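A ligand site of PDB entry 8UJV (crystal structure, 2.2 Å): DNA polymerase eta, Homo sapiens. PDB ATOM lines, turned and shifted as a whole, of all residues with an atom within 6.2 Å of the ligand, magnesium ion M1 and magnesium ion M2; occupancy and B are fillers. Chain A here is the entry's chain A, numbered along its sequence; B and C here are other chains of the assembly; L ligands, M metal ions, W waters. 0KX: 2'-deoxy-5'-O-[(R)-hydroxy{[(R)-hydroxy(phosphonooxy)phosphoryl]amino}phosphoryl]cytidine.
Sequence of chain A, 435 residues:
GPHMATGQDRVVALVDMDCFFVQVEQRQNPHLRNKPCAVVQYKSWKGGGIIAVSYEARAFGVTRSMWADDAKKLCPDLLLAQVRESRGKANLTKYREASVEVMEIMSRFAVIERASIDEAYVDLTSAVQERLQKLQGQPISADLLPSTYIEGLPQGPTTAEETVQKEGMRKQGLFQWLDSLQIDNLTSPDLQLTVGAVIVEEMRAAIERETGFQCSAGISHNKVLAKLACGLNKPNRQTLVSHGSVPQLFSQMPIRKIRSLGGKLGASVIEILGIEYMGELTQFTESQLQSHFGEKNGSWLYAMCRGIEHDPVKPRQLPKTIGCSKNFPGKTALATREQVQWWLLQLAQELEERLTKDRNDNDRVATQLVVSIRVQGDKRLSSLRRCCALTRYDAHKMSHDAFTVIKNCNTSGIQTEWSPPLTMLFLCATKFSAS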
ATOM      1  N   ASP A  16      25.863  24.362  11.245  1.00  0.00           N
ATOM      2  CA  ASP A  16      25.027  24.368  10.052  1.00  0.00           C
ATOM      3  C   ASP A  16      23.557  24.478  10.445  1.00  0.00           C
ATOM      4  O   ASP A  16      23.057  23.659  11.229  1.00  0.00           O
ATOM      5  CB  ASP A  16      25.268  23.109   9.209  1.00  0.00           C
ATOM      6  CG  ASP A  16      24.502  23.134   7.922  1.00  0.00           C
ATOM      7  OD1 ASP A  16      23.283  22.882   7.954  1.00  0.00           O
ATOM      8  OD2 ASP A  16      25.101  23.469   6.872  1.00  0.00           O
ATOM      9  N   MET A  17      22.861  25.461   9.875  1.00  0.00           N
ATOM     10  CA  MET A  17      21.450  25.643  10.191  1.00  0.00           C
ATOM     11  C   MET A  17      20.620  24.477   9.691  1.00  0.00           C
ATOM     12  O   MET A  17      20.852  23.931   8.605  1.00  0.00           O
ATOM     13  CB  MET A  17      20.916  26.941   9.575  1.00  0.00           C
ATOM     14  CG  MET A  17      21.771  28.176   9.813  1.00  0.00           C
ATOM     15  SD  MET A  17      22.133  28.441  11.552  1.00  0.00           S
ATOM     16  CE  MET A  17      20.524  28.833  12.129  1.00  0.00           C
ATOM     17  N   ASP A  18      19.640  24.091  10.498  1.00  0.00           N
ATOM     18  CA  ASP A  18      18.698  23.038  10.129  1.00  0.00           C
ATOM     19  C   ASP A  18      17.684  23.574   9.112  1.00  0.00           C
ATOM     20  O   ASP A  18      17.133  24.661   9.305  1.00  0.00           O
ATOM     21  CB  ASP A  18      18.002  22.511  11.388  1.00  0.00           C
ATOM     22  CG  ASP A  18      18.979  21.971  12.432  1.00  0.00           C
ATOM     23  OD1 ASP A  18      20.047  21.446  12.057  1.00  0.00           O
ATOM     24  OD2 ASP A  18      18.673  22.043  13.639  1.00  0.00           O
ATOM     25  N   CYS A  19      17.442  22.809   8.047  1.00  0.00           N
ATOM     26  CA  CYS A  19      16.582  23.187   6.916  1.00  0.00           C
ATOM     27  C   CYS A  19      16.424  24.695   6.758  1.00  0.00           C
ATOM     28  O   CYS A  19      15.336  25.254   6.954  1.00  0.00           O
ATOM     29  CB  CYS A  19      15.217  22.500   7.060  1.00  0.00           C
ATOM     30  SG  CYS A  19      14.367  22.710   8.668  1.00  0.00           S
ATOM     31  N   PHE A  20      17.515  25.366   6.383  1.00  0.00           N
ATOM     32  CA  PHE A  20      17.656  26.792   6.696  1.00  0.00           C
ATOM     33  C   PHE A  20      16.578  27.661   6.037  1.00  0.00           C
ATOM     34  O   PHE A  20      15.907  28.437   6.704  1.00  0.00           O
ATOM     35  CB  PHE A  20      19.047  27.264   6.291  1.00  0.00           C
ATOM     36  CG  PHE A  20      19.277  28.697   6.570  1.00  0.00           C
ATOM     37  CD1 PHE A  20      18.983  29.232   7.812  1.00  0.00           C
ATOM     38  CD2 PHE A  20      19.748  29.538   5.575  1.00  0.00           C
ATOM     39  CE1 PHE A  20      19.157  30.584   8.076  1.00  0.00           C
ATOM     40  CE2 PHE A  20      19.928  30.899   5.830  1.00  0.00           C
ATOM     41  CZ  PHE A  20      19.642  31.427   7.083  1.00  0.00           C
ATOM     42  N   PHE A  21      16.398  27.537   4.713  1.00  0.00           N
ATOM     43  CA  PHE A  21      15.406  28.375   4.034  1.00  0.00           C
ATOM     44  C   PHE A  21      14.012  28.122   4.592  1.00  0.00           C
ATOM     45  O   PHE A  21      13.214  29.062   4.699  1.00  0.00           O
ATOM     46  CB  PHE A  21      15.422  28.140   2.524  1.00  0.00           C
ATOM     47  CG  PHE A  21      16.599  28.741   1.811  1.00  0.00           C
ATOM     48  CD1 PHE A  21      17.758  29.062   2.493  1.00  0.00           C
ATOM     49  CD2 PHE A  21      16.551  28.976   0.445  1.00  0.00           C
ATOM     50  CE1 PHE A  21      18.841  29.593   1.845  1.00  0.00           C
ATOM     51  CE2 PHE A  21      17.627  29.514  -0.213  1.00  0.00           C
ATOM     52  CZ  PHE A  21      18.785  29.832   0.489  1.00  0.00           C
ATOM     53  N   VAL A  22      13.704  26.878   4.973  1.00  0.00           N
ATOM     54  CA  VAL A  22      12.407  26.586   5.582  1.00  0.00           C
ATOM     55  C   VAL A  22      12.250  27.320   6.902  1.00  0.00           C
ATOM     56  O   VAL A  22      11.214  27.954   7.162  1.00  0.00           O
ATOM     57  CB  VAL A  22      12.228  25.061   5.748  1.00  0.00           C
ATOM     58  CG1 VAL A  22      11.078  24.757   6.678  1.00  0.00           C
ATOM     59  CG2 VAL A  22      11.965  24.422   4.406  1.00  0.00           C
ATOM     60  N   GLN A  41      11.112  27.124  -5.864  1.00  0.00           N
ATOM     61  CA  GLN A  41      11.422  28.139  -6.874  1.00  0.00           C
ATOM     62  C   GLN A  41      10.555  27.903  -8.104  1.00  0.00           C
ATOM     63  O   GLN A  41      10.490  26.780  -8.612  1.00  0.00           O
ATOM     64  CB  GLN A  41      12.884  28.057  -7.324  1.00  0.00           C
ATOM     65  CG  GLN A  41      13.913  28.676  -6.456  1.00  0.00           C
ATOM     66  CD  GLN A  41      15.281  28.295  -6.924  1.00  0.00           C
ATOM     67  OE1 GLN A  41      15.409  27.498  -7.859  1.00  0.00           O
ATOM     68  NE2 GLN A  41      16.316  28.828  -6.269  1.00  0.00           N
ATOM     69  N   ILE A  51      13.977  23.344  -2.922  1.00  0.00           N
ATOM     70  CA  ILE A  51      15.340  23.623  -2.507  1.00  0.00           C
ATOM     71  C   ILE A  51      15.568  23.452  -1.020  1.00  0.00           C
ATOM     72  O   ILE A  51      16.720  23.491  -0.581  1.00  0.00           O
ATOM     73  CB  ILE A  51      15.815  25.029  -2.925  1.00  0.00           C
ATOM     74  CG1 ILE A  51      14.973  26.106  -2.266  1.00  0.00           C
ATOM     75  CG2 ILE A  51      15.781  25.184  -4.443  1.00  0.00           C
ATOM     76  CD1 ILE A  51      15.319  27.503  -2.754  1.00  0.00           C
ATOM     77  N   ALA A  52      14.518  23.321  -0.211  1.00  0.00           N
ATOM     78  CA  ALA A  52      14.713  23.051   1.199  1.00  0.00           C
ATOM     79  C   ALA A  52      13.451  22.405   1.739  1.00  0.00           C
ATOM     80  O   ALA A  52      12.344  22.738   1.305  1.00  0.00           O
ATOM     81  CB  ALA A  52      15.059  24.325   1.978  1.00  0.00           C
ATOM     82  N   VAL A  53      13.644  21.478   2.671  1.00  0.00           N
ATOM     83  CA  VAL A  53      12.597  20.564   3.135  1.00  0.00           C
ATOM     84  C   VAL A  53      12.635  20.505   4.647  1.00  0.00           C
ATOM     85  O   VAL A  53      13.678  20.176   5.229  1.00  0.00           O
ATOM     86  CB  VAL A  53      12.809  19.138   2.580  1.00  0.00           C
ATOM     87  CG1 VAL A  53      11.612  18.259   2.939  1.00  0.00           C
ATOM     88  CG2 VAL A  53      13.046  19.176   1.092  1.00  0.00           C
ATOM     89  N   TYR A  55      12.076  18.870   8.356  1.00  0.00           N
ATOM     90  CA  TYR A  55      12.254  17.484   8.776  1.00  0.00           C
ATOM     91  C   TYR A  55      10.926  16.747   8.855  1.00  0.00           C
ATOM     92  O   TYR A  55      10.916  15.521   8.770  1.00  0.00           O
ATOM     93  CB  TYR A  55      13.001  17.428  10.109  1.00  0.00           C
ATOM     94  CG  TYR A  55      14.482  17.630   9.903  1.00  0.00           C
ATOM     95  CD1 TYR A  55      15.005  18.895   9.740  1.00  0.00           C
ATOM     96  CD2 TYR A  55      15.355  16.551   9.801  1.00  0.00           C
ATOM     97  CE1 TYR A  55      16.351  19.094   9.526  1.00  0.00           C
ATOM     98  CE2 TYR A  55      16.718  16.740   9.576  1.00  0.00           C
ATOM     99  CZ  TYR A  55      17.201  18.015   9.443  1.00  0.00           C
ATOM    100  OH  TYR A  55      18.555  18.244   9.234  1.00  0.00           O
ATOM    101  N   ARG A  58      10.549  15.611   5.310  1.00  0.00           N
ATOM    102  CA  ARG A  58      11.547  14.585   4.991  1.00  0.00           C
ATOM    103  C   ARG A  58      11.066  13.205   5.423  1.00  0.00           C
ATOM    104  O   ARG A  58      11.381  12.206   4.763  1.00  0.00           O
ATOM    105  CB  ARG A  58      12.891  14.895   5.642  1.00  0.00           C
ATOM    106  CG  ARG A  58      13.574  16.183   5.159  1.00  0.00           C
ATOM    107  CD  ARG A  58      14.965  16.402   5.800  1.00  0.00           C
ATOM    108  NE  ARG A  58      15.362  17.799   5.720  1.00  0.00           N
ATOM    109  CZ  ARG A  58      16.588  18.264   5.900  1.00  0.00           C
ATOM    110  NH1 ARG A  58      17.610  17.456   6.170  1.00  0.00           N
ATOM    111  NH2 ARG A  58      16.817  19.573   5.787  1.00  0.00           N
ATOM    112  N   ARG A  64      15.227  17.707  -1.608  1.00  0.00           N
ATOM    113  CA  ARG A  64      15.667  18.780  -2.480  1.00  0.00           C
ATOM    114  C   ARG A  64      15.723  18.298  -3.932  1.00  0.00           C
ATOM    115  O   ARG A  64      15.901  17.108  -4.182  1.00  0.00           O
ATOM    116  CB  ARG A  64      17.060  19.263  -2.024  1.00  0.00           C
ATOM    117  CG  ARG A  64      17.895  19.931  -3.093  1.00  0.00           C
ATOM    118  CD  ARG A  64      19.293  20.294  -2.593  1.00  0.00           C
ATOM    119  NE  ARG A  64      19.210  21.238  -1.491  1.00  0.00           N
ATOM    120  CZ  ARG A  64      19.769  21.054  -0.300  1.00  0.00           C
ATOM    121  NH1 ARG A  64      20.530  19.987  -0.052  1.00  0.00           N
ATOM    122  NH2 ARG A  64      19.576  21.950   0.666  1.00  0.00           N
ATOM    123  N   SER A  65      15.540  19.220  -4.874  1.00  0.00           N
ATOM    124  CA  SER A  65      15.594  18.984  -6.321  1.00  0.00           C
ATOM    125  C   SER A  65      14.398  18.207  -6.848  1.00  0.00           C
ATOM    126  O   SER A  65      14.259  18.050  -8.073  1.00  0.00           O
ATOM    127  CB  SER A  65      16.891  18.264  -6.751  1.00  0.00           C
ATOM    128  OG  SER A  65      18.039  18.996  -6.334  1.00  0.00           O
ATOM    129  N   LEU A  92      17.295  35.724  -3.526  1.00  0.00           N
ATOM    130  CA  LEU A  92      17.608  35.049  -2.278  1.00  0.00           C
ATOM    131  C   LEU A  92      17.901  36.011  -1.141  1.00  0.00           C
ATOM    132  O   LEU A  92      18.424  35.585  -0.098  1.00  0.00           O
ATOM    133  CB  LEU A  92      18.779  34.094  -2.495  1.00  0.00           C
ATOM    134  CG  LEU A  92      18.442  33.084  -3.611  1.00  0.00           C
ATOM    135  CD1 LEU A  92      19.592  32.137  -3.859  1.00  0.00           C
ATOM    136  CD2 LEU A  92      17.161  32.298  -3.305  1.00  0.00           C
ATOM    137  N   SER A 116      29.137  28.737   3.738  1.00  0.00           N
ATOM    138  CA  SER A 116      27.994  28.738   2.840  1.00  0.00           C
ATOM    139  C   SER A 116      26.983  29.711   3.434  1.00  0.00           C
ATOM    140  O   SER A 116      27.219  30.327   4.467  1.00  0.00           O
ATOM    141  CB  SER A 116      27.389  27.352   2.636  1.00  0.00           C
ATOM    142  OG  SER A 116      26.527  26.984   3.705  1.00  0.00           O
ATOM    143  N   ILE A 117      25.831  29.810   2.772  1.00  0.00           N
ATOM    144  CA  ILE A 117      24.799  30.686   3.300  1.00  0.00           C
ATOM    145  C   ILE A 117      24.357  30.243   4.688  1.00  0.00           C
ATOM    146  O   ILE A 117      23.942  31.086   5.501  1.00  0.00           O
ATOM    147  CB  ILE A 117      23.601  30.751   2.327  1.00  0.00           C
ATOM    148  CG1 ILE A 117      22.734  31.971   2.641  1.00  0.00           C
ATOM    149  CG2 ILE A 117      22.805  29.463   2.368  1.00  0.00           C
ATOM    150  CD1 ILE A 117      21.839  32.387   1.503  1.00  0.00           C
ATOM    151  N   ASP A 118      24.460  28.947   5.025  1.00  0.00           N
ATOM    152  CA  ASP A 118      23.938  28.515   6.318  1.00  0.00           C
ATOM    153  C   ASP A 118      24.975  27.805   7.200  1.00  0.00           C
ATOM    154  O   ASP A 118      24.596  27.137   8.175  1.00  0.00           O
ATOM    155  CB  ASP A 118      22.701  27.641   6.139  1.00  0.00           C
ATOM    156  CG  ASP A 118      23.012  26.164   5.957  1.00  0.00           C
ATOM    157  OD1 ASP A 118      23.967  25.848   5.201  1.00  0.00           O
ATOM    158  OD2 ASP A 118      22.314  25.329   6.565  1.00  0.00           O
ATOM    159  N   GLU A 119      26.270  27.950   6.934  1.00  0.00           N
ATOM    160  CA  GLU A 119      27.225  27.297   7.809  1.00  0.00           C
ATOM    161  C   GLU A 119      28.563  28.043   7.845  1.00  0.00           C
ATOM    162  O   GLU A 119      28.947  28.715   6.891  1.00  0.00           O
ATOM    163  CB  GLU A 119      27.466  25.832   7.423  1.00  0.00           C
ATOM    164  CG  GLU A 119      28.104  25.615   6.104  1.00  0.00           C
ATOM    165  CD  GLU A 119      27.595  24.342   5.457  1.00  0.00           C
ATOM    166  OE1 GLU A 119      28.130  23.259   5.770  1.00  0.00           O
ATOM    167  OE2 GLU A 119      26.639  24.416   4.671  1.00  0.00           O
ATOM    168  N   LYS A 234      21.890  15.594  13.407  1.00  0.00           N
ATOM    169  CA  LYS A 234      20.918  16.574  12.952  1.00  0.00           C
ATOM    170  C   LYS A 234      19.501  16.056  13.168  1.00  0.00           C
ATOM    171  O   LYS A 234      19.254  14.859  13.002  1.00  0.00           O
ATOM    172  CB  LYS A 234      21.127  16.875  11.470  1.00  0.00           C
ATOM    173  CG  LYS A 234      22.025  18.041  11.184  1.00  0.00           C
ATOM    174  CD  LYS A 234      21.928  18.440   9.707  1.00  0.00           C
ATOM    175  CE  LYS A 234      22.578  19.826   9.479  1.00  0.00           C
ATOM    176  NZ  LYS A 234      21.731  20.977   9.957  1.00  0.00           N
ATOM    177  N   PRO A 235      18.532  16.927  13.487  1.00  0.00           N
ATOM    178  CA  PRO A 235      18.628  18.383  13.670  1.00  0.00           C
ATOM    179  C   PRO A 235      18.714  18.825  15.145  1.00  0.00           C
ATOM    180  O   PRO A 235      18.468  18.053  16.062  1.00  0.00           O
ATOM    181  CB  PRO A 235      17.334  18.862  13.003  1.00  0.00           C
ATOM    182  CG  PRO A 235      16.334  17.802  13.489  1.00  0.00           C
ATOM    183  CD  PRO A 235      17.116  16.493  13.512  1.00  0.00           C
ATOM    184  P    DT B   8      27.966  19.985   0.941  1.00  0.00           P
ATOM    185  OP1  DT B   8      28.187  19.507   2.323  1.00  0.00           O
ATOM    186  OP2  DT B   8      27.264  19.124  -0.033  1.00  0.00           O
ATOM    187  O5'  DT B   8      27.170  21.394   1.024  1.00  0.00           O
ATOM    188  C5'  DT B   8      27.798  22.561   1.602  1.00  0.00           C
ATOM    189  C4'  DT B   8      26.845  23.744   1.572  1.00  0.00           C
ATOM    190  O4'  DT B   8      26.742  24.237   0.199  1.00  0.00           O
ATOM    191  C3'  DT B   8      25.426  23.407   2.005  1.00  0.00           C
ATOM    192  O3'  DT B   8      24.878  24.485   2.774  1.00  0.00           O
ATOM    193  C2'  DT B   8      24.678  23.193   0.685  1.00  0.00           C
ATOM    194  C1'  DT B   8      25.404  24.157  -0.257  1.00  0.00           C
ATOM    195  N1   DT B   8      25.409  23.704  -1.677  1.00  0.00           N
ATOM    196  C2   DT B   8      25.005  24.589  -2.658  1.00  0.00           C
ATOM    197  O2   DT B   8      24.664  25.735  -2.434  1.00  0.00           O
ATOM    198  N3   DT B   8      25.022  24.075  -3.924  1.00  0.00           N
ATOM    199  C4   DT B   8      25.395  22.825  -4.303  1.00  0.00           C
ATOM    200  O4   DT B   8      25.390  22.469  -5.477  1.00  0.00           O
ATOM    201  C5   DT B   8      25.791  21.941  -3.231  1.00  0.00           C
ATOM    202  C7   DT B   8      26.217  20.532  -3.539  1.00  0.00           C
ATOM    203  C6   DT B   8      25.774  22.421  -1.980  1.00  0.00           C
ATOM    204  N2  XB9 C   4      19.409  26.083  -6.009  1.00  0.00           N
ATOM    205  N1  XB9 C   4      19.894  25.361  -8.148  1.00  0.00           N
ATOM    206  C2  XB9 C   4      20.078  25.276  -6.833  1.00  0.00           C
ATOM    207  O1  XB9 C   4      20.890  24.470  -6.393  1.00  0.00           O
ATOM    208  C1' XB9 C   4      18.940  26.268  -8.743  1.00  0.00           C
ATOM    209  C2' XB9 C   4      19.485  26.718 -10.083  1.00  0.00           C
ATOM    210  C3' XB9 C   4      18.283  26.739 -11.003  1.00  0.00           C
ATOM    211  C4' XB9 C   4      17.322  25.747 -10.362  1.00  0.00           C
ATOM    212  C5' XB9 C   4      17.313  24.433 -11.107  1.00  0.00           C
ATOM    213  O3' XB9 C   4      17.575  27.977 -10.980  1.00  0.00           O
ATOM    214  O4' XB9 C   4      17.778  25.510  -9.033  1.00  0.00           O
ATOM    215  O5' XB9 C   4      17.332  24.749 -12.497  1.00  0.00           O
ATOM    216  OP1 XB9 C   4      16.793  22.608 -13.767  1.00  0.00           O
ATOM    217  P   XB9 C   4      17.855  23.649 -13.514  1.00  0.00           P
ATOM    218  O2  XB9 C   4      18.253  24.324 -14.800  1.00  0.00           O
ATOM    219  P    DA C   5      18.230  29.350 -11.483  1.00  0.00           P
ATOM    220  OP1  DA C   5      17.136  30.329 -11.622  1.00  0.00           O
ATOM    221  OP2  DA C   5      19.106  29.155 -12.673  1.00  0.00           O
ATOM    222  O5'  DA C   5      19.079  29.824 -10.221  1.00  0.00           O
ATOM    223  C5'  DA C   5      18.393  30.154  -9.001  1.00  0.00           C
ATOM    224  C4'  DA C   5      19.368  30.631  -7.953  1.00  0.00           C
ATOM    225  O4'  DA C   5      20.172  29.507  -7.488  1.00  0.00           O
ATOM    226  C3'  DA C   5      20.354  31.688  -8.441  1.00  0.00           C
ATOM    227  O3'  DA C   5      20.534  32.650  -7.413  1.00  0.00           O
ATOM    228  C2'  DA C   5      21.627  30.870  -8.714  1.00  0.00           C
ATOM    229  C1'  DA C   5      21.542  29.810  -7.626  1.00  0.00           C
ATOM    230  N9   DA C   5      22.248  28.566  -7.943  1.00  0.00           N
ATOM    231  C8   DA C   5      22.449  28.019  -9.173  1.00  0.00           C
ATOM    232  N7   DA C   5      23.114  26.874  -9.144  1.00  0.00           N
ATOM    233  C5   DA C   5      23.338  26.669  -7.794  1.00  0.00           C
ATOM    234  C6   DA C   5      23.981  25.635  -7.083  1.00  0.00           C
ATOM    235  N6   DA C   5      24.530  24.584  -7.666  1.00  0.00           N
ATOM    236  N1   DA C   5      24.041  25.741  -5.749  1.00  0.00           N
ATOM    237  C2   DA C   5      23.475  26.801  -5.156  1.00  0.00           C
ATOM    238  N3   DA C   5      22.856  27.828  -5.715  1.00  0.00           N
ATOM    239  C4   DA C   5      22.821  27.705  -7.050  1.00  0.00           C
HETATM  240  PG  0KX L   1      19.864  20.511   6.762  1.00  0.00           P
HETATM  241  O1G 0KX L   1      19.156  20.483   8.082  1.00  0.00           O
HETATM  242  O2G 0KX L   1      21.161  21.245   6.884  1.00  0.00           O
HETATM  243  O3G 0KX L   1      20.057  19.171   6.077  1.00  0.00           O
HETATM  244  PB  0KX L   1      19.325  22.550   4.865  1.00  0.00           P
HETATM  245  O1B 0KX L   1      18.101  23.015   4.079  1.00  0.00           O
HETATM  246  O2B 0KX L   1      19.942  23.651   5.707  1.00  0.00           O
HETATM  247  O3B 0KX L   1      18.836  21.295   5.780  1.00  0.00           O
HETATM  248  PA  0KX L   1      21.917  22.676   3.420  1.00  0.00           P
HETATM  249  O1A 0KX L   1      22.593  22.982   4.709  1.00  0.00           O
HETATM  250  O2A 0KX L   1      22.716  21.780   2.531  1.00  0.00           O
HETATM  251  N3A 0KX L   1      20.479  21.850   3.793  1.00  0.00           N
HETATM  252  O5' 0KX L   1      21.595  24.068   2.567  1.00  0.00           O
HETATM  253  C5' 0KX L   1      21.334  25.251   3.297  1.00  0.00           C
HETATM  254  C4' 0KX L   1      20.299  26.047   2.539  1.00  0.00           C
HETATM  255  O4' 0KX L   1      21.002  26.394   1.174  1.00  0.00           O
HETATM  256  C3' 0KX L   1      19.266  25.290   2.167  1.00  0.00           C
HETATM  257  O3' 0KX L   1      18.174  25.409   3.109  1.00  0.00           O
HETATM  258  C2' 0KX L   1      18.774  25.889   0.735  1.00  0.00           C
HETATM  259  C1' 0KX L   1      19.890  26.411   0.148  1.00  0.00           C
HETATM  260  N1  0KX L   1      20.375  25.596  -0.951  1.00  0.00           N
HETATM  261  C2  0KX L   1      20.055  26.056  -2.332  1.00  0.00           C
HETATM  262  N3  0KX L   1      20.535  25.255  -3.489  1.00  0.00           N
HETATM  263  C4  0KX L   1      21.304  24.040  -3.262  1.00  0.00           C
HETATM  264  C5  0KX L   1      21.626  23.566  -1.874  1.00  0.00           C
HETATM  265  C6  0KX L   1      21.143  24.380  -0.714  1.00  0.00           C
HETATM  266  O2  0KX L   1      19.432  27.035  -2.482  1.00  0.00           O
HETATM  267  N4  0KX L   1      21.750  23.295  -4.394  1.00  0.00           N
HETATM  268 MG    MG M   1      21.807  23.339   6.686  1.00  0.00          MG
HETATM  269 MG    MG M   2      24.547  23.684   4.896  1.00  0.00          MG
HETATM  270  O   HOH W   1      23.325  20.029   6.001  1.00  0.00           O
HETATM  271  O   HOH W   2      25.106  21.669   4.592  1.00  0.00           O
HETATM  272  O   HOH W   3      23.915  26.291   1.516  1.00  0.00           O
HETATM  273  O   HOH W   4      20.237  18.983   3.571  1.00  0.00           O
HETATM  274  O   HOH W   5      22.859  27.976  -1.403  1.00  0.00           O
HETATM  275  O   HOH W   6      18.665  28.432  -4.707  1.00  0.00           O
HETATM  276  O   HOH W   7      16.453  21.216   3.126  1.00  0.00           O
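N3 of DT 8 of chain B is in hydrogen-bond range of a nitrogen (N4) of the ligand (3.4 Å). O1 of XB9 4 of chain C lies within hydrogen-bond range of N4 of the ligand (2.5 Å). OH of Tyr 55 lies within hydrogen-bond range of O1G of the ligand (2.6 Å). The guanidinium group (NH1) of Arg 58 lies within salt-bridge range of an oxygen (O3G) of the ligand (3.0 Å). The backbone NH of Cys 19 sits at hydrogen-bond distance from an oxygen (O1G) of the ligand. The backbone NH (N) of Phe 20 is in hydrogen-bond range of an oxygen (O3') of the ligand (3.3 Å). The side-chain amino group (NZ) of Lys 234 lies within salt-bridge range of an oxygen (O1G) of the ligand (3.2 Å). The backbone NH (N) of Phe 21 is in hydrogen-bond range of an oxygen (O3') of the ligand, 3.2 Å away. NH2 of Arg 64 lies within salt-bridge range of O2A of the ligand (3.7 Å).
The backbone carbonyl oxygen of Asp 16 sits at hydrogen-bond distance from the side-chain amino group of Lys 234, 3.3 Å away. OG of Ser 116 lies close to N of Asp 118 (3.1 Å). The side-chain amino group (NZ) of Lys 234 sits close to the backbone carbonyl oxygen (O) of Met 17. OG of Ser 116 sits close to N of Glu 119. N3 of DT 8 of chain B lies close to N1 of DA 5 of chain C (2.7 Å). O3' of DT 8 of chain B lies close to the side-chain hydroxyl (OG) of Ser 116 (3.1 Å). NE of Arg 58 sits at hydrogen-bond distance from O of Val 53 (3.0 Å). The side-chain carboxylate of Asp 18 is in salt-bridge range of the side-chain amino group of Lys 234, at 2.7 Å.
CA of Asp 18 touches O1G of the ligand, at 3.3 Å. Ile 51 touches the ligand (O to C2', 3.4 Å). CB of Ala 52 touches O3' of the ligand (3.5 Å). CG2 of Ile 117 touches O4' of the ligand, at 3.8 Å. DA 5 of chain C touches the ligand. The nearest printed residue that does not touch the ligand is Glu 119 (4.3 Å).
Within 4 Å of magnesium ion M1: Asp 16, Met 17 and Asp 118. Along chain A the residues within 4 Å of magnesium ion M1 span positions 16 to 118.
Within 4 Å of magnesium ion M2: Asp 16, Asp 118, Glu 119 and DT 8 of chain B. Along chain A the residues within 4 Å of magnesium ion M2 span positions 16 to 119.
Magnesium ion M1 is bound by the side-chain carboxylate of Asp 16 (2.0 Å), the side-chain carboxylate of Asp 118 (2.1 Å), an oxygen (O2B) of the ligand (2.1 Å), an oxygen (O1A) of the ligand (2.2 Å), an oxygen (O2G) of the ligand (2.2 Å) and the backbone carbonyl oxygen of Met 17 (2.2 Å). Magnesium ion M1 has six donor atoms within binding distance.
Magnesium ion M2 is bound by the side-chain carboxylate (OD2) of Asp 16. O1A of the ligand binds magnesium ion M2. Water W2 is bound to magnesium ion M2. OE2 of Glu 119 is bound to magnesium ion M2, at 2.2 Å. OD1 of Asp 118 binds magnesium ion M2. O3' of DT 8 of chain B is bound to magnesium ion M2 (2.3 Å).
Water W7 lies within hydrogen-bond range of an oxygen (O1B) of the ligand (2.6 Å), the backbone NH of Val 53 (2.9 Å) and the guanidinium group of Arg 58 (3.1 Å). Water W6 lies within hydrogen-bond range of an oxygen (O2) of the ligand (2.7 Å), N2 of XB9 4 of chain C (2.8 Å), the side-chain amide nitrogen (NE2) of Gln 41 (2.8 Å) and O4' of DA 5 of chain C (3.3 Å). Water W3 bridges an oxygen (O4') of the ligand (2.9 Å) and the side-chain hydroxyl (OG) of Ser 116 (3.5 Å).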
